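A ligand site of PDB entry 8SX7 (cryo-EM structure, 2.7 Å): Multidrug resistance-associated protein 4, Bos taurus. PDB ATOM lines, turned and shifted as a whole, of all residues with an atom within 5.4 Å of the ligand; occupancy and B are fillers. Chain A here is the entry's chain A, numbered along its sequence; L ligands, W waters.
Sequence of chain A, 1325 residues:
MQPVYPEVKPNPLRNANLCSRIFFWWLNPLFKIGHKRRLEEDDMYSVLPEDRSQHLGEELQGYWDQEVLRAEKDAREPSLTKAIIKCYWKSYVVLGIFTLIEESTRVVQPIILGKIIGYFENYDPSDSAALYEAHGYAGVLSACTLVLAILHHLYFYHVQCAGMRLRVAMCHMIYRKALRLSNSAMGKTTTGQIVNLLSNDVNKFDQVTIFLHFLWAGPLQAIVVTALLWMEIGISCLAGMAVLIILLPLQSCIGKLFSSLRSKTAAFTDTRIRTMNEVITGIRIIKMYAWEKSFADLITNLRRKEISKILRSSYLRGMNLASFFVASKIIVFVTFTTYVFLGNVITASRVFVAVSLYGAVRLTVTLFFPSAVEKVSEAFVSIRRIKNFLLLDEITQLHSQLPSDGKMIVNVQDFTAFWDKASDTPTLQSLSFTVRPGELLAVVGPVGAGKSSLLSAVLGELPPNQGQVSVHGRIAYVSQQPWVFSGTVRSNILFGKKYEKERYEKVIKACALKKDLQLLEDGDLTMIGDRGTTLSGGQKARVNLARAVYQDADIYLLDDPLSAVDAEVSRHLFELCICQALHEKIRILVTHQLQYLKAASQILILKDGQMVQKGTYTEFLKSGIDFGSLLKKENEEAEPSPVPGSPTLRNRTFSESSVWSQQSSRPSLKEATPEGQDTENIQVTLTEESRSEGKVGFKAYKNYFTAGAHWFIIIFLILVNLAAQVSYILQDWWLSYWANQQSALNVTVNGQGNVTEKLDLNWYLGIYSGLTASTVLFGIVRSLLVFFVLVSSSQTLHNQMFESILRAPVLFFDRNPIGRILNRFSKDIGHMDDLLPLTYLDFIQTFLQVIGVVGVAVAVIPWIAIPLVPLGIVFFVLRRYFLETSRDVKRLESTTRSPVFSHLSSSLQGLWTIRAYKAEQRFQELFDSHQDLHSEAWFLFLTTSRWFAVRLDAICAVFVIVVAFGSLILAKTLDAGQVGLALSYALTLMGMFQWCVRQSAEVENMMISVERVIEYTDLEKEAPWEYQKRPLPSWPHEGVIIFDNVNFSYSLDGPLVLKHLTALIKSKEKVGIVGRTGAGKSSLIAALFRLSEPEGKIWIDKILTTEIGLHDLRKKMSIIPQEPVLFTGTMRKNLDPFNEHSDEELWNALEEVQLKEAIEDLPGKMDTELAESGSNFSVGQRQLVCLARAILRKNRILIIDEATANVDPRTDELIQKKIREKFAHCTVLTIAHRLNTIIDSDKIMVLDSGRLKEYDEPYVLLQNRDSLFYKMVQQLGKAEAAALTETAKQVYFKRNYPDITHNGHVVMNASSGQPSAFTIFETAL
Merely in contact with the ligand: Phe 156, Thr 846, Trp 995, Leu 367, Met 992, Phe 324, Phe 368 and Leu 363.
11 residues have an atom within 4 Å of the ligand: Phe 156, Phe 324, Arg 362, Leu 363, Leu 367, Phe 368, Gln 845, Thr 846, Gln 849, Met 992 and Trp 995.
Along chain A the residues within 4 Å of the ligand span positions 156 to 995.
An oxygen (O5) of the ligand lies within hydrogen-bond range of the side-chain amide nitrogen (NE2) of Gln 845, 2.7 Å away.
NE2 of Gln 849 sits at hydrogen-bond distance from O3 of the ligand, 2.8 Å away.
NH2 of Arg 362 is in salt-bridge range of O3 of the ligand (3.7 Å).
Water W1 lies within hydrogen-bond range of an oxygen (O1) of the ligand (2.7 Å), a ring nitrogen (NE2) of His 152 (2.8 Å) and the guanidinium group (NH1) of Arg 946 (3.2 Å).
The backbone carbonyl oxygen (O) of Asp 842 lies within hydrogen-bond range of the side-chain hydroxyl (OG1) of Thr 846, at 2.6 Å.
OD2 of Asp 842 lies within hydrogen-bond range of NE1 of Trp 995, 3.3 Å away.
N of Leu 367 lies within hydrogen-bond range of O of Arg 362 (3.4 Å).
The guanidinium group (NH1) of Arg 362 lies within hydrogen-bond range of the backbone carbonyl oxygen (O) of Phe 325 (3.4 Å).
O of Leu 363 sits at hydrogen-bond distance from N of Phe 368, at 3.0 Å.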
ATOM      1  N   HIS A 152      -8.583 -16.749   6.519  1.00  0.00           N
ATOM      2  CA  HIS A 152      -7.210 -16.390   6.151  1.00  0.00           C
ATOM      3  C   HIS A 152      -6.775 -17.087   4.861  1.00  0.00           C
ATOM      4  O   HIS A 152      -6.308 -16.443   3.921  1.00  0.00           O
ATOM      5  CB  HIS A 152      -6.266 -16.733   7.301  1.00  0.00           C
ATOM      6  CG  HIS A 152      -4.822 -16.556   6.982  1.00  0.00           C
ATOM      7  ND1 HIS A 152      -4.063 -15.549   7.537  1.00  0.00           N
ATOM      8  CD2 HIS A 152      -3.980 -17.262   6.191  1.00  0.00           C
ATOM      9  CE1 HIS A 152      -2.827 -15.633   7.086  1.00  0.00           C
ATOM     10  NE2 HIS A 152      -2.757 -16.664   6.265  1.00  0.00           N
ATOM     11  N   PHE A 156      -6.091 -15.170   1.241  1.00  0.00           N
ATOM     12  CA  PHE A 156      -4.749 -15.119   0.668  1.00  0.00           C
ATOM     13  C   PHE A 156      -4.657 -15.926  -0.608  1.00  0.00           C
ATOM     14  O   PHE A 156      -3.982 -15.524  -1.555  1.00  0.00           O
ATOM     15  CB  PHE A 156      -3.704 -15.516   1.712  1.00  0.00           C
ATOM     16  CG  PHE A 156      -3.373 -14.408   2.651  1.00  0.00           C
ATOM     17  CD1 PHE A 156      -2.607 -13.348   2.208  1.00  0.00           C
ATOM     18  CD2 PHE A 156      -3.874 -14.359   3.925  1.00  0.00           C
ATOM     19  CE1 PHE A 156      -2.308 -12.298   3.024  1.00  0.00           C
ATOM     20  CE2 PHE A 156      -3.572 -13.301   4.756  1.00  0.00           C
ATOM     21  CZ  PHE A 156      -2.794 -12.274   4.302  1.00  0.00           C
ATOM     22  N   ILE A 210      -2.092  -8.261  -2.756  1.00  0.00           N
ATOM     23  CA  ILE A 210      -2.121  -8.982  -1.476  1.00  0.00           C
ATOM     24  C   ILE A 210      -2.712  -8.116  -0.359  1.00  0.00           C
ATOM     25  O   ILE A 210      -3.567  -8.580   0.390  1.00  0.00           O
ATOM     26  CB  ILE A 210      -0.734  -9.541  -1.117  1.00  0.00           C
ATOM     27  CG1 ILE A 210      -0.206 -10.396  -2.269  1.00  0.00           C
ATOM     28  CG2 ILE A 210      -0.762 -10.317   0.171  1.00  0.00           C
ATOM     29  CD1 ILE A 210       1.197 -10.885  -2.071  1.00  0.00           C
ATOM     30  N   PHE A 211      -2.257  -6.877  -0.228  1.00  0.00           N
ATOM     31  CA  PHE A 211      -2.538  -6.058   0.946  1.00  0.00           C
ATOM     32  C   PHE A 211      -3.486  -4.884   0.734  1.00  0.00           C
ATOM     33  O   PHE A 211      -3.705  -4.123   1.680  1.00  0.00           O
ATOM     34  CB  PHE A 211      -1.244  -5.560   1.608  1.00  0.00           C
ATOM     35  CG  PHE A 211      -0.218  -6.627   1.800  1.00  0.00           C
ATOM     36  CD1 PHE A 211      -0.376  -7.549   2.808  1.00  0.00           C
ATOM     37  CD2 PHE A 211       0.890  -6.732   0.987  1.00  0.00           C
ATOM     38  CE1 PHE A 211       0.539  -8.538   3.023  1.00  0.00           C
ATOM     39  CE2 PHE A 211       1.810  -7.731   1.193  1.00  0.00           C
ATOM     40  CZ  PHE A 211       1.633  -8.639   2.210  1.00  0.00           C
ATOM     41  N   PHE A 324       8.260  -2.903  12.826  1.00  0.00           N
ATOM     42  CA  PHE A 324       7.178  -3.871  12.976  1.00  0.00           C
ATOM     43  C   PHE A 324       7.441  -4.811  14.148  1.00  0.00           C
ATOM     44  O   PHE A 324       6.571  -5.004  15.004  1.00  0.00           O
ATOM     45  CB  PHE A 324       6.990  -4.687  11.694  1.00  0.00           C
ATOM     46  CG  PHE A 324       6.288  -5.997  11.934  1.00  0.00           C
ATOM     47  CD1 PHE A 324       4.949  -6.026  12.268  1.00  0.00           C
ATOM     48  CD2 PHE A 324       6.985  -7.191  11.860  1.00  0.00           C
ATOM     49  CE1 PHE A 324       4.314  -7.217  12.504  1.00  0.00           C
ATOM     50  CE2 PHE A 324       6.348  -8.392  12.095  1.00  0.00           C
ATOM     51  CZ  PHE A 324       5.014  -8.400  12.417  1.00  0.00           C
ATOM     52  N   PHE A 325       8.633  -5.400  14.192  1.00  0.00           N
ATOM     53  CA  PHE A 325       8.945  -6.394  15.208  1.00  0.00           C
ATOM     54  C   PHE A 325       8.743  -5.848  16.618  1.00  0.00           C
ATOM     55  O   PHE A 325       8.280  -6.559  17.513  1.00  0.00           O
ATOM     56  CB  PHE A 325      10.375  -6.898  15.011  1.00  0.00           C
ATOM     57  CG  PHE A 325      10.820  -7.917  16.033  1.00  0.00           C
ATOM     58  CD1 PHE A 325      10.318  -9.201  16.017  1.00  0.00           C
ATOM     59  CD2 PHE A 325      11.740  -7.583  17.009  1.00  0.00           C
ATOM     60  CE1 PHE A 325      10.718 -10.135  16.956  1.00  0.00           C
ATOM     61  CE2 PHE A 325      12.143  -8.507  17.949  1.00  0.00           C
ATOM     62  CZ  PHE A 325      11.630  -9.776  17.920  1.00  0.00           C
ATOM     63  N   ARG A 362      -1.173  -4.563  15.241  1.00  0.00           N
ATOM     64  CA  ARG A 362       0.214  -4.654  14.785  1.00  0.00           C
ATOM     65  C   ARG A 362       0.267  -5.213  13.370  1.00  0.00           C
ATOM     66  O   ARG A 362       0.870  -4.611  12.470  1.00  0.00           O
ATOM     67  CB  ARG A 362       1.041  -5.495  15.752  1.00  0.00           C
ATOM     68  CG  ARG A 362       2.532  -5.392  15.502  1.00  0.00           C
ATOM     69  CD  ARG A 362       3.365  -6.286  16.398  1.00  0.00           C
ATOM     70  NE  ARG A 362       3.293  -7.699  16.045  1.00  0.00           N
ATOM     71  CZ  ARG A 362       4.316  -8.544  16.066  1.00  0.00           C
ATOM     72  NH1 ARG A 362       5.534  -8.148  16.399  1.00  0.00           N
ATOM     73  NH2 ARG A 362       4.113  -9.813  15.751  1.00  0.00           N
ATOM     74  N   LEU A 363      -0.308  -6.400  13.158  1.00  0.00           N
ATOM     75  CA  LEU A 363      -0.323  -6.972  11.819  1.00  0.00           C
ATOM     76  C   LEU A 363      -0.879  -5.986  10.791  1.00  0.00           C
ATOM     77  O   LEU A 363      -0.205  -5.613   9.833  1.00  0.00           O
ATOM     78  CB  LEU A 363      -1.122  -8.274  11.809  1.00  0.00           C
ATOM     79  CG  LEU A 363      -0.602  -9.417  12.680  1.00  0.00           C
ATOM     80  CD1 LEU A 363      -1.399 -10.671  12.397  1.00  0.00           C
ATOM     81  CD2 LEU A 363       0.887  -9.665  12.483  1.00  0.00           C
ATOM     82  N   LEU A 367       2.198  -3.657   9.541  1.00  0.00           N
ATOM     83  CA  LEU A 367       2.798  -4.555   8.562  1.00  0.00           C
ATOM     84  C   LEU A 367       2.103  -4.478   7.211  1.00  0.00           C
ATOM     85  O   LEU A 367       2.767  -4.252   6.205  1.00  0.00           O
ATOM     86  CB  LEU A 367       2.804  -5.996   9.091  1.00  0.00           C
ATOM     87  CG  LEU A 367       3.400  -7.078   8.174  1.00  0.00           C
ATOM     88  CD1 LEU A 367       4.902  -6.944   8.057  1.00  0.00           C
ATOM     89  CD2 LEU A 367       3.023  -8.448   8.684  1.00  0.00           C
ATOM     90  N   PHE A 368       0.780  -4.648   7.170  1.00  0.00           N
ATOM     91  CA  PHE A 368       0.088  -4.790   5.889  1.00  0.00           C
ATOM     92  C   PHE A 368      -0.165  -3.446   5.242  1.00  0.00           C
ATOM     93  O   PHE A 368      -0.143  -3.345   4.015  1.00  0.00           O
ATOM     94  CB  PHE A 368      -1.235  -5.533   6.071  1.00  0.00           C
ATOM     95  CG  PHE A 368      -1.094  -6.982   6.480  1.00  0.00           C
ATOM     96  CD1 PHE A 368       0.034  -7.714   6.169  1.00  0.00           C
ATOM     97  CD2 PHE A 368      -2.112  -7.595   7.185  1.00  0.00           C
ATOM     98  CE1 PHE A 368       0.151  -9.028   6.553  1.00  0.00           C
ATOM     99  CE2 PHE A 368      -2.004  -8.918   7.575  1.00  0.00           C
ATOM    100  CZ  PHE A 368      -0.871  -9.629   7.252  1.00  0.00           C
ATOM    101  N   ASP A 842      13.790 -12.637   7.964  1.00  0.00           N
ATOM    102  CA  ASP A 842      12.427 -13.141   8.149  1.00  0.00           C
ATOM    103  C   ASP A 842      12.421 -14.498   8.853  1.00  0.00           C
ATOM    104  O   ASP A 842      11.746 -14.681   9.871  1.00  0.00           O
ATOM    105  CB  ASP A 842      11.729 -13.220   6.798  1.00  0.00           C
ATOM    106  CG  ASP A 842      10.224 -13.282   6.932  1.00  0.00           C
ATOM    107  OD1 ASP A 842       9.732 -13.717   7.991  1.00  0.00           O
ATOM    108  OD2 ASP A 842       9.528 -12.895   5.978  1.00  0.00           O
ATOM    109  N   GLN A 845      13.830 -14.376  12.471  1.00  0.00           N
ATOM    110  CA  GLN A 845      12.845 -13.750  13.356  1.00  0.00           C
ATOM    111  C   GLN A 845      11.694 -14.711  13.662  1.00  0.00           C
ATOM    112  O   GLN A 845      11.293 -14.860  14.819  1.00  0.00           O
ATOM    113  CB  GLN A 845      12.343 -12.466  12.711  1.00  0.00           C
ATOM    114  CG  GLN A 845      11.327 -11.697  13.521  1.00  0.00           C
ATOM    115  CD  GLN A 845      10.980 -10.379  12.869  1.00  0.00           C
ATOM    116  OE1 GLN A 845      11.781  -9.461  12.857  1.00  0.00           O
ATOM    117  NE2 GLN A 845       9.780 -10.299  12.300  1.00  0.00           N
ATOM    118  N   THR A 846      11.132 -15.349  12.624  1.00  0.00           N
ATOM    119  CA  THR A 846       9.996 -16.247  12.825  1.00  0.00           C
ATOM    120  C   THR A 846      10.394 -17.517  13.563  1.00  0.00           C
ATOM    121  O   THR A 846       9.640 -18.020  14.402  1.00  0.00           O
ATOM    122  CB  THR A 846       9.364 -16.606  11.488  1.00  0.00           C
ATOM    123  OG1 THR A 846       9.381 -15.478  10.611  1.00  0.00           O
ATOM    124  CG2 THR A 846       7.918 -17.007  11.692  1.00  0.00           C
ATOM    125  N   GLN A 849      10.660 -16.817  17.200  1.00  0.00           N
ATOM    126  CA  GLN A 849       9.308 -16.652  17.738  1.00  0.00           C
ATOM    127  C   GLN A 849       8.662 -18.003  18.024  1.00  0.00           C
ATOM    128  O   GLN A 849       8.057 -18.200  19.085  1.00  0.00           O
ATOM    129  CB  GLN A 849       8.455 -15.854  16.751  1.00  0.00           C
ATOM    130  CG  GLN A 849       8.852 -14.401  16.573  1.00  0.00           C
ATOM    131  CD  GLN A 849       8.292 -13.527  17.649  1.00  0.00           C
ATOM    132  OE1 GLN A 849       8.620 -13.680  18.819  1.00  0.00           O
ATOM    133  NE2 GLN A 849       7.456 -12.587  17.266  1.00  0.00           N
ATOM    134  N   ARG A 946      -0.665 -23.921  -0.353  1.00  0.00           N
ATOM    135  CA  ARG A 946      -1.857 -23.864   0.509  1.00  0.00           C
ATOM    136  C   ARG A 946      -2.151 -25.204   1.181  1.00  0.00           C
ATOM    137  O   ARG A 946      -2.490 -25.227   2.370  1.00  0.00           O
ATOM    138  CB  ARG A 946      -3.082 -23.413  -0.282  1.00  0.00           C
ATOM    139  CG  ARG A 946      -3.088 -21.953  -0.645  1.00  0.00           C
ATOM    140  CD  ARG A 946      -3.225 -21.031   0.560  1.00  0.00           C
ATOM    141  NE  ARG A 946      -2.540 -19.783   0.268  1.00  0.00           N
ATOM    142  CZ  ARG A 946      -1.899 -19.028   1.144  1.00  0.00           C
ATOM    143  NH1 ARG A 946      -2.031 -19.215   2.444  1.00  0.00           N
ATOM    144  NH2 ARG A 946      -1.149 -18.028   0.707  1.00  0.00           N
ATOM    145  N   GLY A 991      -0.502 -18.958  11.648  1.00  0.00           N
ATOM    146  CA  GLY A 991       0.143 -18.133  10.650  1.00  0.00           C
ATOM    147  C   GLY A 991       1.640 -18.005  10.810  1.00  0.00           C
ATOM    148  O   GLY A 991       2.383 -18.096   9.835  1.00  0.00           O
ATOM    149  N   MET A 992       2.106 -17.776  12.041  1.00  0.00           N
ATOM    150  CA  MET A 992       3.533 -17.696  12.308  1.00  0.00           C
ATOM    151  C   MET A 992       4.251 -18.991  11.942  1.00  0.00           C
ATOM    152  O   MET A 992       5.236 -18.979  11.192  1.00  0.00           O
ATOM    153  CB  MET A 992       3.750 -17.340  13.772  1.00  0.00           C
ATOM    154  CG  MET A 992       5.207 -17.326  14.230  1.00  0.00           C
ATOM    155  SD  MET A 992       5.358 -17.691  15.982  1.00  0.00           S
ATOM    156  CE  MET A 992       4.814 -16.143  16.684  1.00  0.00           C
ATOM    157  N   GLN A 994       3.466 -21.739  10.149  1.00  0.00           N
ATOM    158  CA  GLN A 994       3.482 -22.101   8.731  1.00  0.00           C
ATOM    159  C   GLN A 994       4.331 -21.145   7.904  1.00  0.00           C
ATOM    160  O   GLN A 994       5.011 -21.568   6.962  1.00  0.00           O
ATOM    161  CB  GLN A 994       2.034 -22.246   8.227  1.00  0.00           C
ATOM    162  CG  GLN A 994       1.121 -21.037   8.299  1.00  0.00           C
ATOM    163  CD  GLN A 994       1.117 -20.165   7.052  1.00  0.00           C
ATOM    164  OE1 GLN A 994       1.796 -20.446   6.065  1.00  0.00           O
ATOM    165  NE2 GLN A 994       0.307 -19.124   7.089  1.00  0.00           N
ATOM    166  N   TRP A 995       4.301 -19.845   8.212  1.00  0.00           N
ATOM    167  CA  TRP A 995       5.196 -18.893   7.557  1.00  0.00           C
ATOM    168  C   TRP A 995       6.664 -19.221   7.827  1.00  0.00           C
ATOM    169  O   TRP A 995       7.499 -19.188   6.913  1.00  0.00           O
ATOM    170  CB  TRP A 995       4.834 -17.471   7.989  1.00  0.00           C
ATOM    171  CG  TRP A 995       5.545 -16.403   7.210  1.00  0.00           C
ATOM    172  CD1 TRP A 995       6.498 -15.547   7.664  1.00  0.00           C
ATOM    173  CD2 TRP A 995       5.409 -16.142   5.808  1.00  0.00           C
ATOM    174  NE1 TRP A 995       6.922 -14.725   6.647  1.00  0.00           N
ATOM    175  CE2 TRP A 995       6.278 -15.085   5.495  1.00  0.00           C
ATOM    176  CE3 TRP A 995       4.632 -16.684   4.787  1.00  0.00           C
ATOM    177  CZ2 TRP A 995       6.394 -14.563   4.211  1.00  0.00           C
ATOM    178  CZ3 TRP A 995       4.734 -16.160   3.517  1.00  0.00           C
ATOM    179  CH2 TRP A 995       5.609 -15.109   3.238  1.00  0.00           C
ATOM    180  N   ARG A 998       7.569 -22.475   5.657  1.00  0.00           N
ATOM    181  CA  ARG A 998       7.716 -22.160   4.232  1.00  0.00           C
ATOM    182  C   ARG A 998       8.845 -21.176   3.957  1.00  0.00           C
ATOM    183  O   ARG A 998       9.471 -21.235   2.891  1.00  0.00           O
ATOM    184  CB  ARG A 998       6.388 -21.669   3.644  1.00  0.00           C
ATOM    185  CG  ARG A 998       5.302 -22.732   3.660  1.00  0.00           C
ATOM    186  CD  ARG A 998       3.994 -22.300   3.014  1.00  0.00           C
ATOM    187  NE  ARG A 998       3.378 -21.167   3.681  1.00  0.00           N
ATOM    188  CZ  ARG A 998       2.751 -20.166   3.060  1.00  0.00           C
ATOM    189  NH1 ARG A 998       2.643 -20.114   1.752  1.00  0.00           N
ATOM    190  NH2 ARG A 998       2.201 -19.206   3.797  1.00  0.00           N
HETATM  191  C1  LIG L   1       0.372 -12.957   5.507  1.00  0.00           C
HETATM  192  C2  LIG L   1       1.511 -13.844   5.240  1.00  0.00           C
HETATM  193  C3  LIG L   1       1.518 -14.972   6.224  1.00  0.00           C
HETATM  194  C4  LIG L   1       1.819 -14.595   7.600  1.00  0.00           C
HETATM  195  C5  LIG L   1       2.950 -13.632   7.850  1.00  0.00           C
HETATM  196  C6  LIG L   1       3.181 -12.622   6.747  1.00  0.00           C
HETATM  197  C7  LIG L   1       2.844 -13.138   5.381  1.00  0.00           C
HETATM  198  C8  LIG L   1       2.988 -12.370   4.151  1.00  0.00           C
HETATM  199  C9  LIG L   1       2.323 -13.128   3.124  1.00  0.00           C
HETATM  200  C10 LIG L   1       1.504 -14.151   3.779  1.00  0.00           C
HETATM  201  C11 LIG L   1       4.491 -11.999   6.848  1.00  0.00           C
HETATM  202  C12 LIG L   1       4.925 -11.698   8.153  1.00  0.00           C
HETATM  203  C13 LIG L   1       4.401 -12.121   9.263  1.00  0.00           C
HETATM  204  C14 LIG L   1       3.180 -13.054   9.272  1.00  0.00           C
HETATM  205  C15 LIG L   1       3.456 -14.133  10.290  1.00  0.00           C
HETATM  206  C16 LIG L   1       3.944 -13.710  11.590  1.00  0.00           C
HETATM  207  C17 LIG L   1       5.102 -12.823  11.581  1.00  0.00           C
HETATM  208  C18 LIG L   1       4.928 -11.774  10.583  1.00  0.00           C
HETATM  209  C19 LIG L   1       1.998 -12.315   9.712  1.00  0.00           C
HETATM  210  O1  LIG L   1       0.925 -15.084   3.251  1.00  0.00           O
HETATM  211  O2  LIG L   1       5.397 -12.347  12.784  1.00  0.00           O
HETATM  212  O3  LIG L   1       6.881 -11.969  14.561  1.00  0.00           O
HETATM  213  O4  LIG L   1       6.956 -14.034  13.432  1.00  0.00           O
HETATM  214  O5  LIG L   1       7.777 -12.075  12.346  1.00  0.00           O
HETATM  215  S1  LIG L   1       6.860 -12.624  13.297  1.00  0.00           S
HETATM  216  O   HOH W   1      -0.917 -16.774   4.175  1.00  0.00           O
